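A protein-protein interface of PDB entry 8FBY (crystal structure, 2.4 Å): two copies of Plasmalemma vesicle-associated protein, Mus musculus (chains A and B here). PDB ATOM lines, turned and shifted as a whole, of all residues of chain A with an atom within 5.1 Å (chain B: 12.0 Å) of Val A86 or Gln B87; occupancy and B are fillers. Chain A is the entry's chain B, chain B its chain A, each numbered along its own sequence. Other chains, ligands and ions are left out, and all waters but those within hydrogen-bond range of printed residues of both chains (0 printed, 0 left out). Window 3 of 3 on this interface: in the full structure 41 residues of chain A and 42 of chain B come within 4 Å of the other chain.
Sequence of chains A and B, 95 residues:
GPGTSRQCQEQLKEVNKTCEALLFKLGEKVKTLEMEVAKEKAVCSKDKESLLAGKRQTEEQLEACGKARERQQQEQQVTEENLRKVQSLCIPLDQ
Of the 16 printed residues of chain B, 5 touch a printed residue of chain A. Hydrophobic or aromatic side chains of chain B that line the printed part of chain A: Leu B83 and Val B86. Of the 9 printed residues of chain A, 4 touch a printed residue of chain B. Among the printed residues, no Asp or Glu carboxylate lies within 4 Å of a Lys or Arg side-chain nitrogen of the other chain.
The side-chain sulfur (SG) of Cys B90 is disulfide-bonded to the side-chain sulfur (SG) of Cys A90, at 2.0 Å.
Leu A83 touches its own counterpart, Leu B83. Val A86 touches its own counterpart, Val B86. Val A86 touches Gln B87, but with the chains exchanged Gln A87 does not touch Val B86 (4.3 Å). Cys A90 touches its own counterpart, Cys B90. Positions printed for both chains: 82, 83, 84, 85, 86, 87, 88, 89 and 90. Of the 7 pairs that touch across the chains among the printed residues, 5 have their exchanged pair printed and touching as well.
Asn A82 touches Leu B83. ND2 of Asn B82 touches CD2 of Leu A83, at 3.4 Å. Leu B83 touches Leu A83. Val A86 touches Leu B83 (CG1 to CD1, 3.8 Å). CG1 of Val A86 touches CG1 of Val B86 (3.6 Å). Val A86 touches Gln B87 (CG2 to CG, 3.6 Å).
Of chain B, only Leu B83, Val B86 and Gln B87 come within 4 Å of Val A86. Of the printed residues of chain A, Gln B87 touches Val A86 (3.6 Å). Leu A83 touches two residues of chain B. No residue of chain B comes within 4 Å of Gln A87. No residue of chain B comes within 4 Å of Ser A88. Cys A90 touches one residue of chain B. Of the printed residues of chain A, Leu B83 touches Asn A82, Leu A83 and Val A86. Printed residues of chain A within 4 Å of Val B86: Val A86. Of the printed residues of chain A, Cys B90 touches Cys A90. The nearest printed residue of chain A that does not touch Gln B87 is Asn A82 (5.2 Å).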
ATOM      1  N   ASN A  82       4.980 -17.755  14.885  1.00  0.00           N
ATOM      2  CA  ASN A  82       5.998 -18.407  15.716  1.00  0.00           C
ATOM      3  C   ASN A  82       5.444 -19.725  16.273  1.00  0.00           C
ATOM      4  O   ASN A  82       6.167 -20.721  16.304  1.00  0.00           O
ATOM      5  CB  ASN A  82       6.415 -17.504  16.885  1.00  0.00           C
ATOM      6  CG  ASN A  82       7.251 -16.319  16.525  1.00  0.00           C
ATOM      7  OD1 ASN A  82       7.765 -16.189  15.402  1.00  0.00           O
ATOM      8  ND2 ASN A  82       7.395 -15.430  17.495  1.00  0.00           N
ATOM      9  N   LEU A  83       4.168 -19.722  16.719  1.00  0.00           N
ATOM     10  CA  LEU A  83       3.499 -20.905  17.246  1.00  0.00           C
ATOM     11  C   LEU A  83       3.414 -21.994  16.175  1.00  0.00           C
ATOM     12  O   LEU A  83       3.763 -23.135  16.446  1.00  0.00           O
ATOM     13  CB  LEU A  83       2.103 -20.542  17.824  1.00  0.00           C
ATOM     14  CG  LEU A  83       1.259 -21.687  18.410  1.00  0.00           C
ATOM     15  CD1 LEU A  83       1.954 -22.358  19.596  1.00  0.00           C
ATOM     16  CD2 LEU A  83      -0.107 -21.195  18.820  1.00  0.00           C
ATOM     17  N   ARG A  84       3.004 -21.636  14.963  1.00  0.00           N
ATOM     18  CA  ARG A  84       2.903 -22.542  13.812  1.00  0.00           C
ATOM     19  C   ARG A  84       4.269 -23.172  13.485  1.00  0.00           C
ATOM     20  O   ARG A  84       4.338 -24.377  13.236  1.00  0.00           O
ATOM     21  CB  ARG A  84       2.404 -21.776  12.583  1.00  0.00           C
ATOM     22  CG  ARG A  84       0.912 -21.665  12.458  1.00  0.00           C
ATOM     23  CD  ARG A  84       0.525 -21.278  11.039  1.00  0.00           C
ATOM     24  NE  ARG A  84       0.899 -19.907  10.698  1.00  0.00           N
ATOM     25  CZ  ARG A  84       0.128 -18.844  10.904  1.00  0.00           C
ATOM     26  NH1 ARG A  84      -1.067 -18.979  11.466  1.00  0.00           N
ATOM     27  NH2 ARG A  84       0.551 -17.636  10.559  1.00  0.00           N
ATOM     28  N   LYS A  85       5.350 -22.355  13.501  1.00  0.00           N
ATOM     29  CA  LYS A  85       6.724 -22.805  13.207  1.00  0.00           C
ATOM     30  C   LYS A  85       7.308 -23.703  14.290  1.00  0.00           C
ATOM     31  O   LYS A  85       7.965 -24.687  13.959  1.00  0.00           O
ATOM     32  CB  LYS A  85       7.662 -21.624  12.892  1.00  0.00           C
ATOM     33  CG  LYS A  85       7.376 -21.017  11.520  1.00  0.00           C
ATOM     34  CD  LYS A  85       8.069 -19.687  11.330  1.00  0.00           C
ATOM     35  CE  LYS A  85       8.628 -19.538   9.940  1.00  0.00           C
ATOM     36  NZ  LYS A  85       9.243 -18.203   9.745  1.00  0.00           N
ATOM     37  N   VAL A  86       7.069 -23.384  15.570  1.00  0.00           N
ATOM     38  CA  VAL A  86       7.555 -24.186  16.684  1.00  0.00           C
ATOM     39  C   VAL A  86       6.777 -25.515  16.815  1.00  0.00           C
ATOM     40  O   VAL A  86       7.383 -26.507  17.204  1.00  0.00           O
ATOM     41  CB  VAL A  86       7.630 -23.382  18.003  1.00  0.00           C
ATOM     42  CG1 VAL A  86       6.305 -23.300  18.728  1.00  0.00           C
ATOM     43  CG2 VAL A  86       8.701 -23.942  18.913  1.00  0.00           C
ATOM     44  N   GLN A  87       5.513 -25.527  16.416  1.00  0.00           N
ATOM     45  CA  GLN A  87       4.683 -26.745  16.499  1.00  0.00           C
ATOM     46  C   GLN A  87       5.221 -27.833  15.568  1.00  0.00           C
ATOM     47  O   GLN A  87       5.099 -28.981  15.933  1.00  0.00           O
ATOM     48  CB  GLN A  87       3.211 -26.411  16.297  1.00  0.00           C
ATOM     49  CG  GLN A  87       2.369 -26.743  17.512  1.00  0.00           C
ATOM     50  CD  GLN A  87       1.149 -25.876  17.680  1.00  0.00           C
ATOM     51  OE1 GLN A  87       0.762 -25.132  16.793  1.00  0.00           O
ATOM     52  NE2 GLN A  87       0.526 -25.967  18.839  1.00  0.00           N
ATOM     53  N   SER A  88       5.792 -27.466  14.422  1.00  0.00           N
ATOM     54  CA  SER A  88       6.399 -28.406  13.475  1.00  0.00           C
ATOM     55  C   SER A  88       7.609 -29.149  14.053  1.00  0.00           C
ATOM     56  O   SER A  88       7.870 -30.255  13.612  1.00  0.00           O
ATOM     57  CB  SER A  88       6.762 -27.712  12.164  1.00  0.00           C
ATOM     58  OG  SER A  88       7.840 -26.805  12.303  1.00  0.00           O
ATOM     59  N   LEU A  89       8.244 -28.577  15.075  1.00  0.00           N
ATOM     60  CA  LEU A  89       9.429 -29.164  15.745  1.00  0.00           C
ATOM     61  C   LEU A  89       9.025 -29.952  16.992  1.00  0.00           C
ATOM     62  O   LEU A  89       9.833 -30.736  17.435  1.00  0.00           O
ATOM     63  CB  LEU A  89      10.346 -28.029  16.201  1.00  0.00           C
ATOM     64  CG  LEU A  89      11.045 -27.229  15.113  1.00  0.00           C
ATOM     65  CD1 LEU A  89      11.828 -26.089  15.721  1.00  0.00           C
ATOM     66  CD2 LEU A  89      11.953 -28.123  14.304  1.00  0.00           C
ATOM     67  N   CYS A  90       7.815 -29.770  17.512  1.00  0.00           N
ATOM     68  CA  CYS A  90       7.479 -30.380  18.822  1.00  0.00           C
ATOM     69  C   CYS A  90       6.248 -31.285  18.803  1.00  0.00           C
ATOM     70  O   CYS A  90       5.258 -30.927  18.175  1.00  0.00           O
ATOM     71  CB  CYS A  90       7.214 -29.287  19.847  1.00  0.00           C
ATOM     72  SG  CYS A  90       8.298 -27.848  19.698  1.00  0.00           S
ATOM     73  N   GLN B  76      -3.570 -11.600  23.027  1.00  0.00           N
ATOM     74  CA  GLN B  76      -2.110 -11.628  22.898  1.00  0.00           C
ATOM     75  C   GLN B  76      -1.456 -12.333  24.098  1.00  0.00           C
ATOM     76  O   GLN B  76      -0.567 -13.161  23.888  1.00  0.00           O
ATOM     77  CB  GLN B  76      -1.542 -10.201  22.686  1.00  0.00           C
ATOM     78  CG  GLN B  76       0.000 -10.079  22.658  1.00  0.00           C
ATOM     79  CD  GLN B  76       0.690 -10.773  21.496  1.00  0.00           C
ATOM     80  OE1 GLN B  76       0.141 -10.911  20.398  1.00  0.00           O
ATOM     81  NE2 GLN B  76       1.924 -11.214  21.722  1.00  0.00           N
ATOM     82  N   VAL B  78      -2.726 -14.622  26.071  1.00  0.00           N
ATOM     83  CA  VAL B  78      -3.098 -16.038  25.961  1.00  0.00           C
ATOM     84  C   VAL B  78      -2.210 -16.765  24.938  1.00  0.00           C
ATOM     85  O   VAL B  78      -1.654 -17.822  25.249  1.00  0.00           O
ATOM     86  CB  VAL B  78      -4.622 -16.190  25.660  1.00  0.00           C
ATOM     87  CG1 VAL B  78      -4.987 -17.609  25.218  1.00  0.00           C
ATOM     88  CG2 VAL B  78      -5.460 -15.769  26.863  1.00  0.00           C
ATOM     89  N   THR B  79      -2.076 -16.185  23.723  1.00  0.00           N
ATOM     90  CA  THR B  79      -1.272 -16.717  22.620  1.00  0.00           C
ATOM     91  C   THR B  79       0.195 -16.805  23.017  1.00  0.00           C
ATOM     92  O   THR B  79       0.842 -17.818  22.726  1.00  0.00           O
ATOM     93  CB  THR B  79      -1.496 -15.894  21.332  1.00  0.00           C
ATOM     94  OG1 THR B  79      -2.892 -15.663  21.176  1.00  0.00           O
ATOM     95  CG2 THR B  79      -0.995 -16.606  20.083  1.00  0.00           C
ATOM     96  N   GLU B  80       0.694 -15.753  23.716  1.00  0.00           N
ATOM     97  CA  GLU B  80       2.079 -15.652  24.166  1.00  0.00           C
ATOM     98  C   GLU B  80       2.437 -16.740  25.167  1.00  0.00           C
ATOM     99  O   GLU B  80       3.508 -17.337  25.045  1.00  0.00           O
ATOM    100  CB  GLU B  80       2.399 -14.250  24.701  1.00  0.00           C
ATOM    101  CG  GLU B  80       3.889 -13.945  24.800  1.00  0.00           C
ATOM    102  CD  GLU B  80       4.705 -14.232  23.550  1.00  0.00           C
ATOM    103  OE1 GLU B  80       5.555 -15.153  23.594  1.00  0.00           O
ATOM    104  OE2 GLU B  80       4.484 -13.547  22.524  1.00  0.00           O
ATOM    105  N   GLU B  81       1.525 -17.010  26.129  1.00  0.00           N
ATOM    106  CA  GLU B  81       1.676 -18.045  27.148  1.00  0.00           C
ATOM    107  C   GLU B  81       1.668 -19.430  26.490  1.00  0.00           C
ATOM    108  O   GLU B  81       2.516 -20.261  26.829  1.00  0.00           O
ATOM    109  CB  GLU B  81       0.566 -17.935  28.201  1.00  0.00           C
ATOM    110  CG  GLU B  81       1.017 -17.277  29.500  1.00  0.00           C
ATOM    111  CD  GLU B  81      -0.107 -16.729  30.362  1.00  0.00           C
ATOM    112  OE1 GLU B  81      -1.112 -17.450  30.568  1.00  0.00           O
ATOM    113  OE2 GLU B  81       0.019 -15.576  30.839  1.00  0.00           O
ATOM    114  N   ASN B  82       0.746 -19.661  25.520  1.00  0.00           N
ATOM    115  CA  ASN B  82       0.675 -20.923  24.778  1.00  0.00           C
ATOM    116  C   ASN B  82       2.013 -21.175  24.037  1.00  0.00           C
ATOM    117  O   ASN B  82       2.546 -22.291  24.082  1.00  0.00           O
ATOM    118  CB  ASN B  82      -0.507 -20.906  23.810  1.00  0.00           C
ATOM    119  CG  ASN B  82      -0.701 -22.147  22.968  1.00  0.00           C
ATOM    120  OD1 ASN B  82      -0.237 -23.243  23.285  1.00  0.00           O
ATOM    121  ND2 ASN B  82      -1.421 -22.004  21.867  1.00  0.00           N
ATOM    122  N   LEU B  83       2.564 -20.128  23.406  1.00  0.00           N
ATOM    123  CA  LEU B  83       3.848 -20.192  22.720  1.00  0.00           C
ATOM    124  C   LEU B  83       4.985 -20.541  23.711  1.00  0.00           C
ATOM    125  O   LEU B  83       5.784 -21.430  23.421  1.00  0.00           O
ATOM    126  CB  LEU B  83       4.125 -18.883  21.945  1.00  0.00           C
ATOM    127  CG  LEU B  83       5.476 -18.772  21.226  1.00  0.00           C
ATOM    128  CD1 LEU B  83       5.619 -19.827  20.137  1.00  0.00           C
ATOM    129  CD2 LEU B  83       5.697 -17.348  20.697  1.00  0.00           C
ATOM    130  N   ARG B  84       5.004 -19.914  24.905  1.00  0.00           N
ATOM    131  CA  ARG B  84       6.031 -20.215  25.920  1.00  0.00           C
ATOM    132  C   ARG B  84       5.901 -21.655  26.418  1.00  0.00           C
ATOM    133  O   ARG B  84       6.913 -22.355  26.537  1.00  0.00           O
ATOM    134  CB  ARG B  84       6.028 -19.183  27.079  1.00  0.00           C
ATOM    135  CG  ARG B  84       6.311 -17.745  26.604  1.00  0.00           C
ATOM    136  CD  ARG B  84       7.061 -16.876  27.601  1.00  0.00           C
ATOM    137  NE  ARG B  84       8.492 -16.844  27.287  1.00  0.00           N
ATOM    138  CZ  ARG B  84       9.475 -16.879  28.186  1.00  0.00           C
ATOM    139  NH1 ARG B  84      10.739 -16.883  27.791  1.00  0.00           N
ATOM    140  NH2 ARG B  84       9.199 -16.919  29.486  1.00  0.00           N
ATOM    141  N   LYS B  85       4.651 -22.113  26.646  1.00  0.00           N
ATOM    142  CA  LYS B  85       4.332 -23.467  27.082  1.00  0.00           C
ATOM    143  C   LYS B  85       4.849 -24.509  26.076  1.00  0.00           C
ATOM    144  O   LYS B  85       5.599 -25.423  26.465  1.00  0.00           O
ATOM    145  CB  LYS B  85       2.810 -23.622  27.289  1.00  0.00           C
ATOM    146  CG  LYS B  85       2.463 -24.944  27.955  1.00  0.00           C
ATOM    147  CD  LYS B  85       0.986 -25.210  28.024  1.00  0.00           C
ATOM    148  CE  LYS B  85       0.750 -26.458  28.859  1.00  0.00           C
ATOM    149  NZ  LYS B  85      -0.682 -26.602  29.226  1.00  0.00           N
ATOM    150  N   VAL B  86       4.494 -24.334  24.806  1.00  0.00           N
ATOM    151  CA  VAL B  86       4.930 -25.249  23.715  1.00  0.00           C
ATOM    152  C   VAL B  86       6.457 -25.231  23.602  1.00  0.00           C
ATOM    153  O   VAL B  86       7.015 -26.273  23.363  1.00  0.00           O
ATOM    154  CB  VAL B  86       4.260 -24.889  22.376  1.00  0.00           C
ATOM    155  CG1 VAL B  86       4.933 -25.542  21.187  1.00  0.00           C
ATOM    156  CG2 VAL B  86       2.778 -25.195  22.390  1.00  0.00           C
ATOM    157  N   GLN B  87       7.092 -24.083  23.784  1.00  0.00           N
ATOM    158  CA  GLN B  87       8.563 -23.998  23.658  1.00  0.00           C
ATOM    159  C   GLN B  87       9.254 -24.653  24.860  1.00  0.00           C
ATOM    160  O   GLN B  87      10.314 -25.224  24.666  1.00  0.00           O
ATOM    161  CB  GLN B  87       8.998 -22.553  23.426  1.00  0.00           C
ATOM    162  CG  GLN B  87       8.764 -22.092  22.006  1.00  0.00           C
ATOM    163  CD  GLN B  87       9.338 -20.740  21.680  1.00  0.00           C
ATOM    164  OE1 GLN B  87       9.718 -19.971  22.542  1.00  0.00           O
ATOM    165  NE2 GLN B  87       9.400 -20.442  20.404  1.00  0.00           N
ATOM    166  N   SER B  88       8.660 -24.564  26.044  1.00  0.00           N
ATOM    167  CA  SER B  88       9.243 -25.160  27.271  1.00  0.00           C
ATOM    168  C   SER B  88       9.106 -26.676  27.249  1.00  0.00           C
ATOM    169  O   SER B  88      10.020 -27.342  27.690  1.00  0.00           O
ATOM    170  CB  SER B  88       8.582 -24.636  28.489  1.00  0.00           C
ATOM    171  OG  SER B  88       8.619 -23.239  28.504  1.00  0.00           O
ATOM    172  N   LEU B  89       7.982 -27.166  26.742  1.00  0.00           N
ATOM    173  CA  LEU B  89       7.712 -28.618  26.752  1.00  0.00           C
ATOM    174  C   LEU B  89       8.250 -29.273  25.488  1.00  0.00           C
ATOM    175  O   LEU B  89       8.255 -30.478  25.436  1.00  0.00           O
ATOM    176  CB  LEU B  89       6.215 -28.847  26.952  1.00  0.00           C
ATOM    177  CG  LEU B  89       5.696 -28.405  28.315  1.00  0.00           C
ATOM    178  CD1 LEU B  89       4.242 -28.755  28.494  1.00  0.00           C
ATOM    179  CD2 LEU B  89       6.528 -28.989  29.435  1.00  0.00           C
ATOM    180  N   CYS B  90       8.690 -28.476  24.526  1.00  0.00           N
ATOM    181  CA  CYS B  90       9.277 -29.014  23.278  1.00  0.00           C
ATOM    182  C   CYS B  90      10.528 -29.807  23.649  1.00  0.00           C
ATOM    183  O   CYS B  90      11.302 -29.310  24.470  1.00  0.00           O
ATOM    184  CB  CYS B  90       9.668 -27.867  22.362  1.00  0.00           C
ATOM    185  SG  CYS B  90       9.965 -28.342  20.646  1.00  0.00           S
ATOM    186  N   ILE B  91      10.669 -31.008  23.097  1.00  0.00           N
ATOM    187  CA  ILE B  91      11.844 -31.900  23.322  1.00  0.00           C
ATOM    188  C   ILE B  91      12.031 -32.213  24.805  1.00  0.00           C
ATOM    189  O   ILE B  91      12.948 -31.676  25.396  1.00  0.00           O
ATOM    190  CB  ILE B  91      13.138 -31.299  22.751  1.00  0.00           C
ATOM    191  CG1 ILE B  91      13.034 -30.953  21.267  1.00  0.00           C
ATOM    192  CG2 ILE B  91      14.295 -32.220  23.056  1.00  0.00           C
ATOM    193  CD1 ILE B  91      14.114 -30.029  20.798  1.00  0.00           C
ATOM    194  N   PRO B  92      11.284 -33.153  25.403  1.00  0.00           N
ATOM    195  CA  PRO B  92      11.459 -33.479  26.813  1.00  0.00           C
ATOM    196  C   PRO B  92      12.833 -34.095  27.116  1.00  0.00           C
ATOM    197  O   PRO B  92      13.379 -34.743  26.246  1.00  0.00           O
ATOM    198  CB  PRO B  92      10.394 -34.545  27.068  1.00  0.00           C
ATOM    199  CG  PRO B  92       9.419 -34.371  25.939  1.00  0.00           C
ATOM    200  CD  PRO B  92      10.254 -33.933  24.760  1.00  0.00           C
